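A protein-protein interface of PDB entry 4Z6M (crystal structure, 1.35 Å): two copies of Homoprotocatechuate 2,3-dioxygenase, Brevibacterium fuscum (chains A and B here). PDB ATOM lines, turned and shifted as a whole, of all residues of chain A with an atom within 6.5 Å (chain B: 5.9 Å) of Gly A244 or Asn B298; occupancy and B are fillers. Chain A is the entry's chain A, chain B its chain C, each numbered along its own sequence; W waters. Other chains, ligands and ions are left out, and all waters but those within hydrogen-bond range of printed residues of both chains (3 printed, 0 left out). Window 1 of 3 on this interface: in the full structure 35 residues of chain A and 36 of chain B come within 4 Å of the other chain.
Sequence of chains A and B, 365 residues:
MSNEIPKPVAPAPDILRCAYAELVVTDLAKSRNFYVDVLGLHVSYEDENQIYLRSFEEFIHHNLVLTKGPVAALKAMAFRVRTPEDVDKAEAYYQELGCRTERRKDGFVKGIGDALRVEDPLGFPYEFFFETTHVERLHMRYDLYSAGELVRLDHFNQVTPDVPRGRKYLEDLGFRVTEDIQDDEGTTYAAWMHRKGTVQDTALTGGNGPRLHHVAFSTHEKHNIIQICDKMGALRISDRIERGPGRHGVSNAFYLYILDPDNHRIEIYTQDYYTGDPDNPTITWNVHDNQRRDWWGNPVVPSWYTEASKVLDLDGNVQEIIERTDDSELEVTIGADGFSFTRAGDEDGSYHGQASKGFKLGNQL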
ATOM      1  N   CYS A 229      28.711 -19.960 -24.109  1.00  0.00           N
ATOM      2  CA  CYS A 229      29.060 -21.351 -24.368  1.00  0.00           C
ATOM      3  C   CYS A 229      29.877 -21.522 -25.634  1.00  0.00           C
ATOM      4  O   CYS A 229      30.924 -22.181 -25.636  1.00  0.00           O
ATOM      5  CB  CYS A 229      27.784 -22.202 -24.470  1.00  0.00           C
ATOM      6  SG  CYS A 229      26.767 -22.239 -23.003  1.00  0.00           S
ATOM      7  N   SER A 238      35.780 -25.600 -22.743  1.00  0.00           N
ATOM      8  CA  SER A 238      34.436 -26.129 -22.482  1.00  0.00           C
ATOM      9  C   SER A 238      34.390 -26.946 -21.195  1.00  0.00           C
ATOM     10  O   SER A 238      33.313 -27.145 -20.631  1.00  0.00           O
ATOM     11  CB  SER A 238      33.903 -26.957 -23.655  1.00  0.00           C
ATOM     12  OG  SER A 238      34.760 -28.053 -23.942  1.00  0.00           O
ATOM     13  N   ILE A 241      32.693 -25.088 -18.501  1.00  0.00           N
ATOM     14  CA  ILE A 241      31.226 -25.049 -18.487  1.00  0.00           C
ATOM     15  C   ILE A 241      30.770 -26.192 -17.596  1.00  0.00           C
ATOM     16  O   ILE A 241      30.969 -27.359 -17.926  1.00  0.00           O
ATOM     17  CB  ILE A 241      30.638 -25.230 -19.889  1.00  0.00           C
ATOM     18  CG1 ILE A 241      31.100 -24.123 -20.840  1.00  0.00           C
ATOM     19  CG2 ILE A 241      29.115 -25.308 -19.832  1.00  0.00           C
ATOM     20  CD1 ILE A 241      30.732 -24.354 -22.279  1.00  0.00           C
ATOM     21  N   GLU A 242      30.214 -25.854 -16.440  1.00  0.00           N
ATOM     22  CA  GLU A 242      29.887 -26.888 -15.457  1.00  0.00           C
ATOM     23  C   GLU A 242      28.548 -27.545 -15.784  1.00  0.00           C
ATOM     24  O   GLU A 242      28.420 -28.763 -15.685  1.00  0.00           O
ATOM     25  CB  GLU A 242      29.838 -26.285 -14.045  1.00  0.00           C
ATOM     26  CG  GLU A 242      29.696 -27.344 -12.963  1.00  0.00           C
ATOM     27  CD  GLU A 242      29.246 -26.817 -11.622  1.00  0.00           C
ATOM     28  OE1 GLU A 242      28.571 -25.792 -11.578  1.00  0.00           O
ATOM     29  OE2 GLU A 242      29.597 -27.463 -10.604  1.00  0.00           O
ATOM     30  N   ARG A 243      27.543 -26.732 -16.109  1.00  0.00           N
ATOM     31  CA  ARG A 243      26.168 -27.218 -16.197  1.00  0.00           C
ATOM     32  C   ARG A 243      25.371 -26.241 -17.030  1.00  0.00           C
ATOM     33  O   ARG A 243      25.409 -25.032 -16.786  1.00  0.00           O
ATOM     34  CB  ARG A 243      25.557 -27.304 -14.803  1.00  0.00           C
ATOM     35  CG  ARG A 243      24.080 -27.652 -14.768  1.00  0.00           C
ATOM     36  CD  ARG A 243      23.498 -27.696 -13.367  1.00  0.00           C
ATOM     37  NE  ARG A 243      22.053 -27.652 -13.514  1.00  0.00           N
ATOM     38  CZ  ARG A 243      21.202 -27.030 -12.705  1.00  0.00           C
ATOM     39  NH1 ARG A 243      21.597 -26.566 -11.532  1.00  0.00           N
ATOM     40  NH2 ARG A 243      19.939 -26.938 -13.065  1.00  0.00           N
ATOM     41  N   GLY A 244      24.610 -26.775 -17.970  1.00  0.00           N
ATOM     42  CA  GLY A 244      23.731 -25.963 -18.802  1.00  0.00           C
ATOM     43  C   GLY A 244      24.228 -25.916 -20.240  1.00  0.00           C
ATOM     44  O   GLY A 244      25.078 -26.717 -20.653  1.00  0.00           O
ATOM     45  N   PRO A 245      23.679 -24.999 -21.031  1.00  0.00           N
ATOM     46  CA  PRO A 245      22.629 -24.061 -20.665  1.00  0.00           C
ATOM     47  C   PRO A 245      21.272 -24.762 -20.496  1.00  0.00           C
ATOM     48  O   PRO A 245      21.076 -25.865 -20.985  1.00  0.00           O
ATOM     49  CB  PRO A 245      22.605 -23.096 -21.840  1.00  0.00           C
ATOM     50  CG  PRO A 245      23.003 -23.937 -22.993  1.00  0.00           C
ATOM     51  CD  PRO A 245      23.998 -24.927 -22.452  1.00  0.00           C
ATOM     52  N   GLY A 246      20.371 -24.134 -19.762  1.00  0.00           N
ATOM     53  CA  GLY A 246      19.042 -24.695 -19.584  1.00  0.00           C
ATOM     54  C   GLY A 246      18.014 -23.642 -19.282  1.00  0.00           C
ATOM     55  O   GLY A 246      18.290 -22.452 -19.243  1.00  0.00           O
ATOM     56  N   TYR A 255      19.581 -20.196 -18.087  1.00  0.00           N
ATOM     57  CA  TYR A 255      20.754 -20.212 -17.220  1.00  0.00           C
ATOM     58  C   TYR A 255      21.935 -20.960 -17.804  1.00  0.00           C
ATOM     59  O   TYR A 255      21.803 -21.782 -18.731  1.00  0.00           O
ATOM     60  CB  TYR A 255      20.388 -20.850 -15.870  1.00  0.00           C
ATOM     61  CG  TYR A 255      20.238 -22.355 -15.912  1.00  0.00           C
ATOM     62  CD1 TYR A 255      21.327 -23.182 -15.773  1.00  0.00           C
ATOM     63  CD2 TYR A 255      18.994 -22.966 -16.103  1.00  0.00           C
ATOM     64  CE1 TYR A 255      21.218 -24.559 -15.822  1.00  0.00           C
ATOM     65  CE2 TYR A 255      18.871 -24.345 -16.149  1.00  0.00           C
ATOM     66  CZ  TYR A 255      19.983 -25.146 -16.022  1.00  0.00           C
ATOM     67  OH  TYR A 255      19.865 -26.521 -16.027  1.00  0.00           O
ATOM     68  N   LEU A 256      23.084 -20.712 -17.165  1.00  0.00           N
ATOM     69  CA  LEU A 256      24.337 -21.385 -17.458  1.00  0.00           C
ATOM     70  C   LEU A 256      25.209 -21.293 -16.217  1.00  0.00           C
ATOM     71  O   LEU A 256      25.214 -20.245 -15.581  1.00  0.00           O
ATOM     72  CB  LEU A 256      25.061 -20.693 -18.619  1.00  0.00           C
ATOM     73  CG  LEU A 256      26.428 -21.263 -19.028  1.00  0.00           C
ATOM     74  CD1 LEU A 256      26.305 -22.674 -19.573  1.00  0.00           C
ATOM     75  CD2 LEU A 256      27.113 -20.320 -19.982  1.00  0.00           C
ATOM     76  N   TYR A 257      25.938 -22.356 -15.865  1.00  0.00           N
ATOM     77  CA  TYR A 257      26.943 -22.265 -14.803  1.00  0.00           C
ATOM     78  C   TYR A 257      28.338 -22.555 -15.354  1.00  0.00           C
ATOM     79  O   TYR A 257      28.548 -23.568 -16.019  1.00  0.00           O
ATOM     80  CB  TYR A 257      26.653 -23.245 -13.658  1.00  0.00           C
ATOM     81  CG  TYR A 257      25.313 -23.014 -13.000  1.00  0.00           C
ATOM     82  CD1 TYR A 257      25.138 -22.094 -11.967  1.00  0.00           C
ATOM     83  CD2 TYR A 257      24.187 -23.712 -13.449  1.00  0.00           C
ATOM     84  CE1 TYR A 257      23.904 -21.905 -11.376  1.00  0.00           C
ATOM     85  CE2 TYR A 257      22.969 -23.515 -12.877  1.00  0.00           C
ATOM     86  CZ  TYR A 257      22.826 -22.616 -11.845  1.00  0.00           C
ATOM     87  OH  TYR A 257      21.590 -22.458 -11.312  1.00  0.00           O
ATOM     88  N   ASP A 294      16.183 -28.126 -13.874  1.00  0.00           N
ATOM     89  CA  ASP A 294      16.176 -27.995 -15.328  1.00  0.00           C
ATOM     90  C   ASP A 294      14.799 -28.408 -15.814  1.00  0.00           C
ATOM     91  O   ASP A 294      14.407 -29.573 -15.696  1.00  0.00           O
ATOM     92  CB  ASP A 294      17.277 -28.826 -15.993  1.00  0.00           C
ATOM     93  CG  ASP A 294      17.415 -28.484 -17.429  1.00  0.00           C
ATOM     94  OD1 ASP A 294      18.062 -27.439 -17.730  1.00  0.00           O
ATOM     95  OD2 ASP A 294      16.824 -29.185 -18.264  1.00  0.00           O
ATOM     96  N   VAL A 301      24.373 -31.847 -12.797  1.00  0.00           N
ATOM     97  CA  VAL A 301      25.701 -32.391 -12.666  1.00  0.00           C
ATOM     98  C   VAL A 301      26.079 -32.510 -11.177  1.00  0.00           C
ATOM     99  O   VAL A 301      25.761 -31.644 -10.371  1.00  0.00           O
ATOM    100  CB  VAL A 301      26.729 -31.526 -13.445  1.00  0.00           C
ATOM    101  CG1 VAL A 301      26.298 -31.315 -14.892  1.00  0.00           C
ATOM    102  CG2 VAL A 301      26.969 -30.217 -12.752  1.00  0.00           C
ATOM    103  N   PRO B 245      19.170 -29.018 -25.613  1.00  0.00           N
ATOM    104  CA  PRO B 245      19.705 -28.410 -26.820  1.00  0.00           C
ATOM    105  C   PRO B 245      21.209 -28.178 -26.716  1.00  0.00           C
ATOM    106  O   PRO B 245      21.785 -28.150 -25.621  1.00  0.00           O
ATOM    107  CB  PRO B 245      18.938 -27.081 -26.894  1.00  0.00           C
ATOM    108  CG  PRO B 245      18.729 -26.726 -25.452  1.00  0.00           C
ATOM    109  CD  PRO B 245      18.508 -28.041 -24.738  1.00  0.00           C
ATOM    110  N   TYR B 255      21.074 -27.303 -32.075  1.00  0.00           N
ATOM    111  CA  TYR B 255      20.340 -28.568 -32.267  1.00  0.00           C
ATOM    112  C   TYR B 255      19.565 -29.010 -31.046  1.00  0.00           C
ATOM    113  O   TYR B 255      19.823 -28.566 -29.928  1.00  0.00           O
ATOM    114  CB  TYR B 255      21.294 -29.716 -32.652  1.00  0.00           C
ATOM    115  CG  TYR B 255      22.129 -30.231 -31.496  1.00  0.00           C
ATOM    116  CD1 TYR B 255      21.645 -31.215 -30.638  1.00  0.00           C
ATOM    117  CD2 TYR B 255      23.391 -29.741 -31.258  1.00  0.00           C
ATOM    118  CE1 TYR B 255      22.402 -31.681 -29.578  1.00  0.00           C
ATOM    119  CE2 TYR B 255      24.148 -30.179 -30.202  1.00  0.00           C
ATOM    120  CZ  TYR B 255      23.655 -31.168 -29.372  1.00  0.00           C
ATOM    121  OH  TYR B 255      24.412 -31.652 -28.317  1.00  0.00           O
ATOM    122  N   ASN B 290      35.983 -34.163 -27.380  1.00  0.00           N
ATOM    123  CA  ASN B 290      34.713 -33.974 -26.684  1.00  0.00           C
ATOM    124  C   ASN B 290      33.911 -32.747 -27.122  1.00  0.00           C
ATOM    125  O   ASN B 290      32.832 -32.516 -26.584  1.00  0.00           O
ATOM    126  CB  ASN B 290      34.944 -33.916 -25.167  1.00  0.00           C
ATOM    127  CG  ASN B 290      33.677 -34.041 -24.383  1.00  0.00           C
ATOM    128  OD1 ASN B 290      32.913 -35.005 -24.564  1.00  0.00           O
ATOM    129  ND2 ASN B 290      33.437 -33.075 -23.496  1.00  0.00           N
ATOM    130  N   ASP B 294      28.849 -32.243 -29.295  1.00  0.00           N
ATOM    131  CA  ASP B 294      28.391 -31.063 -28.576  1.00  0.00           C
ATOM    132  C   ASP B 294      29.609 -30.193 -28.312  1.00  0.00           C
ATOM    133  O   ASP B 294      30.542 -30.588 -27.594  1.00  0.00           O
ATOM    134  CB  ASP B 294      27.708 -31.435 -27.268  1.00  0.00           C
ATOM    135  CG  ASP B 294      27.036 -30.237 -26.627  1.00  0.00           C
ATOM    136  OD1 ASP B 294      25.905 -29.893 -27.080  1.00  0.00           O
ATOM    137  OD2 ASP B 294      27.680 -29.601 -25.771  1.00  0.00           O
ATOM    138  N   TRP B 295      29.608 -29.027 -28.933  1.00  0.00           N
ATOM    139  CA  TRP B 295      30.712 -28.079 -28.878  1.00  0.00           C
ATOM    140  C   TRP B 295      31.020 -27.579 -27.473  1.00  0.00           C
ATOM    141  O   TRP B 295      32.151 -27.167 -27.196  1.00  0.00           O
ATOM    142  CB  TRP B 295      30.342 -26.925 -29.817  1.00  0.00           C
ATOM    143  CG  TRP B 295      31.302 -25.781 -29.964  1.00  0.00           C
ATOM    144  CD1 TRP B 295      31.072 -24.492 -29.646  1.00  0.00           C
ATOM    145  CD2 TRP B 295      32.589 -25.827 -30.568  1.00  0.00           C
ATOM    146  NE1 TRP B 295      32.152 -23.705 -30.004  1.00  0.00           N
ATOM    147  CE2 TRP B 295      33.100 -24.505 -30.568  1.00  0.00           C
ATOM    148  CE3 TRP B 295      33.372 -26.858 -31.105  1.00  0.00           C
ATOM    149  CZ2 TRP B 295      34.327 -24.186 -31.103  1.00  0.00           C
ATOM    150  CZ3 TRP B 295      34.623 -26.541 -31.605  1.00  0.00           C
ATOM    151  CH2 TRP B 295      35.089 -25.226 -31.604  1.00  0.00           C
ATOM    152  N   TRP B 296      30.013 -27.644 -26.591  1.00  0.00           N
ATOM    153  CA  TRP B 296      30.129 -27.192 -25.216  1.00  0.00           C
ATOM    154  C   TRP B 296      30.589 -28.313 -24.297  1.00  0.00           C
ATOM    155  O   TRP B 296      30.760 -28.111 -23.076  1.00  0.00           O
ATOM    156  CB  TRP B 296      28.808 -26.630 -24.731  1.00  0.00           C
ATOM    157  CG  TRP B 296      28.205 -25.618 -25.669  1.00  0.00           C
ATOM    158  CD1 TRP B 296      28.856 -24.775 -26.521  1.00  0.00           C
ATOM    159  CD2 TRP B 296      26.810 -25.357 -25.835  1.00  0.00           C
ATOM    160  NE1 TRP B 296      27.943 -23.980 -27.183  1.00  0.00           N
ATOM    161  CE2 TRP B 296      26.680 -24.327 -26.792  1.00  0.00           C
ATOM    162  CE3 TRP B 296      25.651 -25.892 -25.268  1.00  0.00           C
ATOM    163  CZ2 TRP B 296      25.444 -23.824 -27.196  1.00  0.00           C
ATOM    164  CZ3 TRP B 296      24.420 -25.382 -25.673  1.00  0.00           C
ATOM    165  CH2 TRP B 296      24.334 -24.380 -26.636  1.00  0.00           C
ATOM    166  N   GLY B 297      30.831 -29.479 -24.895  1.00  0.00           N
ATOM    167  CA  GLY B 297      31.344 -30.624 -24.175  1.00  0.00           C
ATOM    168  C   GLY B 297      30.296 -31.400 -23.413  1.00  0.00           C
ATOM    169  O   GLY B 297      30.647 -32.298 -22.634  1.00  0.00           O
ATOM    170  N   ASN B 298      29.022 -31.042 -23.549  1.00  0.00           N
ATOM    171  CA  ASN B 298      27.999 -31.829 -22.875  1.00  0.00           C
ATOM    172  C   ASN B 298      28.011 -33.275 -23.366  1.00  0.00           C
ATOM    173  O   ASN B 298      28.313 -33.543 -24.537  1.00  0.00           O
ATOM    174  CB  ASN B 298      26.607 -31.198 -22.997  1.00  0.00           C
ATOM    175  CG  ASN B 298      26.400 -30.054 -22.025  1.00  0.00           C
ATOM    176  OD1 ASN B 298      26.892 -30.094 -20.897  1.00  0.00           O
ATOM    177  ND2 ASN B 298      25.682 -29.025 -22.460  1.00  0.00           N
ATOM    178  N   PRO B 299      27.695 -34.222 -22.468  1.00  0.00           N
ATOM    179  CA  PRO B 299      27.846 -35.617 -22.844  1.00  0.00           C
ATOM    180  C   PRO B 299      26.781 -36.053 -23.830  1.00  0.00           C
ATOM    181  O   PRO B 299      25.654 -35.557 -23.804  1.00  0.00           O
ATOM    182  CB  PRO B 299      27.690 -36.349 -21.510  1.00  0.00           C
ATOM    183  CG  PRO B 299      26.819 -35.447 -20.700  1.00  0.00           C
ATOM    184  CD  PRO B 299      27.250 -34.065 -21.072  1.00  0.00           C
ATOM    185  N   VAL B 300      27.146 -36.981 -24.704  1.00  0.00           N
ATOM    186  CA  VAL B 300      26.199 -37.565 -25.657  1.00  0.00           C
ATOM    187  C   VAL B 300      25.446 -38.684 -24.958  1.00  0.00           C
ATOM    188  O   VAL B 300      26.034 -39.648 -24.507  1.00  0.00           O
ATOM    189  CB  VAL B 300      26.867 -38.070 -26.949  1.00  0.00           C
ATOM    190  CG1 VAL B 300      25.828 -38.692 -27.868  1.00  0.00           C
ATOM    191  CG2 VAL B 300      27.632 -36.958 -27.637  1.00  0.00           C
ATOM    192  N   SER B 356      31.626 -36.797 -19.977  1.00  0.00           N
ATOM    193  CA  SER B 356      31.905 -35.485 -19.439  1.00  0.00           C
ATOM    194  C   SER B 356      30.906 -35.073 -18.357  1.00  0.00           C
ATOM    195  O   SER B 356      29.872 -35.717 -18.143  1.00  0.00           O
ATOM    196  CB  SER B 356      31.868 -34.479 -20.581  1.00  0.00           C
ATOM    197  OG  SER B 356      30.591 -34.543 -21.195  1.00  0.00           O
ATOM    198  N   LYS B 357      31.236 -33.974 -17.686  1.00  0.00           N
ATOM    199  CA  LYS B 357      30.368 -33.255 -16.746  1.00  0.00           C
ATOM    200  C   LYS B 357      29.981 -34.084 -15.520  1.00  0.00           C
ATOM    201  O   LYS B 357      29.003 -33.773 -14.835  1.00  0.00           O
ATOM    202  CB  LYS B 357      29.104 -32.724 -17.432  1.00  0.00           C
ATOM    203  CG  LYS B 357      29.291 -31.985 -18.760  1.00  0.00           C
ATOM    204  CD  LYS B 357      30.169 -30.743 -18.734  1.00  0.00           C
ATOM    205  CE  LYS B 357      30.085 -29.997 -20.066  1.00  0.00           C
ATOM    206  NZ  LYS B 357      31.245 -29.069 -20.274  1.00  0.00           N
HETATM  207  O   HOH W   1      25.340 -29.474 -18.677  1.00  0.00           O
HETATM  208  O   HOH W   2      21.750 -28.059 -22.751  1.00  0.00           O
HETATM  209  O   HOH W   3      34.950 -30.639 -22.982  1.00  0.00           O
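O of Gly A244 sits at hydrogen-bond distance from ND2 of Asn B298 (3.0 Å). The backbone carbonyl oxygen of Ile A241 lies within hydrogen-bond range of the side-chain amino group of Lys B357. NZ of Lys B357 lies within hydrogen-bond range of O of Ser A238 (2.8 Å).
OD2 of Asp B294 lies close to N of Trp B296, 3.2 Å away. The backbone carbonyl oxygen (O) of Trp B296 is in hydrogen-bond range of the side-chain amino group (NZ) of Lys B357, at 3.0 Å. The side-chain carboxylate (OD2) of Asp B294 sits at hydrogen-bond distance from the backbone NH (N) of Asn B298.
Positions printed for both chains: 245, 255 and 294.
Water W3 lies within hydrogen-bond range of OG of Ser A238 (2.8 Å) and ND2 of Asn B290 (2.9 Å). Water W1 bridges OD1 of Asn B298 (2.8 Å) and N of Gly A244 (2.9 Å). Water W2 bridges O of Pro B245 and O of Pro A245.
Of the 13 printed residues of chain A, 6 touch a printed residue of chain B. Hydrophobic or aromatic side chains of chain A that line the printed part of chain B: Ile A241, Pro A245 and Val A301. Of the 12 printed residues of chain B, 4 touch a printed residue of chain A. Hydrophobic or aromatic side chains of chain B within 4 Å of the printed part of chain A: Trp B296. Among the printed residues, 9 pairs touch across the chains.
Glu A242 touches none of the printed residues of chain B. Of the printed residues of chain A, Trp B296 touches Cys A229, Ser A238, Ile A241 and Pro A245. Of chain A, only Gly A244 comes within 4 Å of Asn B298. Printed residues of chain A within 4 Å of Lys B357: Ser A238 (2.8 Å), Ile A241 (2.9 Å) and Val A301 (3.5 Å). The nearest printed residue of chain A that does not touch Trp B296 is Gly A244 (4.7 Å).
NE1 of Trp B296 touches CB of Cys A229 (3.2 Å). Ser A238 touches Trp B295 (CB to O, 3.96 Å). Ser A238 touches Trp B296 (CB to O, 3.4 Å). Trp B296 touches Ile A241 (O to CD1, 3.8 Å). Trp B296 touches Pro A245 (CZ3 to CD, 3.3 Å). Lys B357 touches Val A301.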
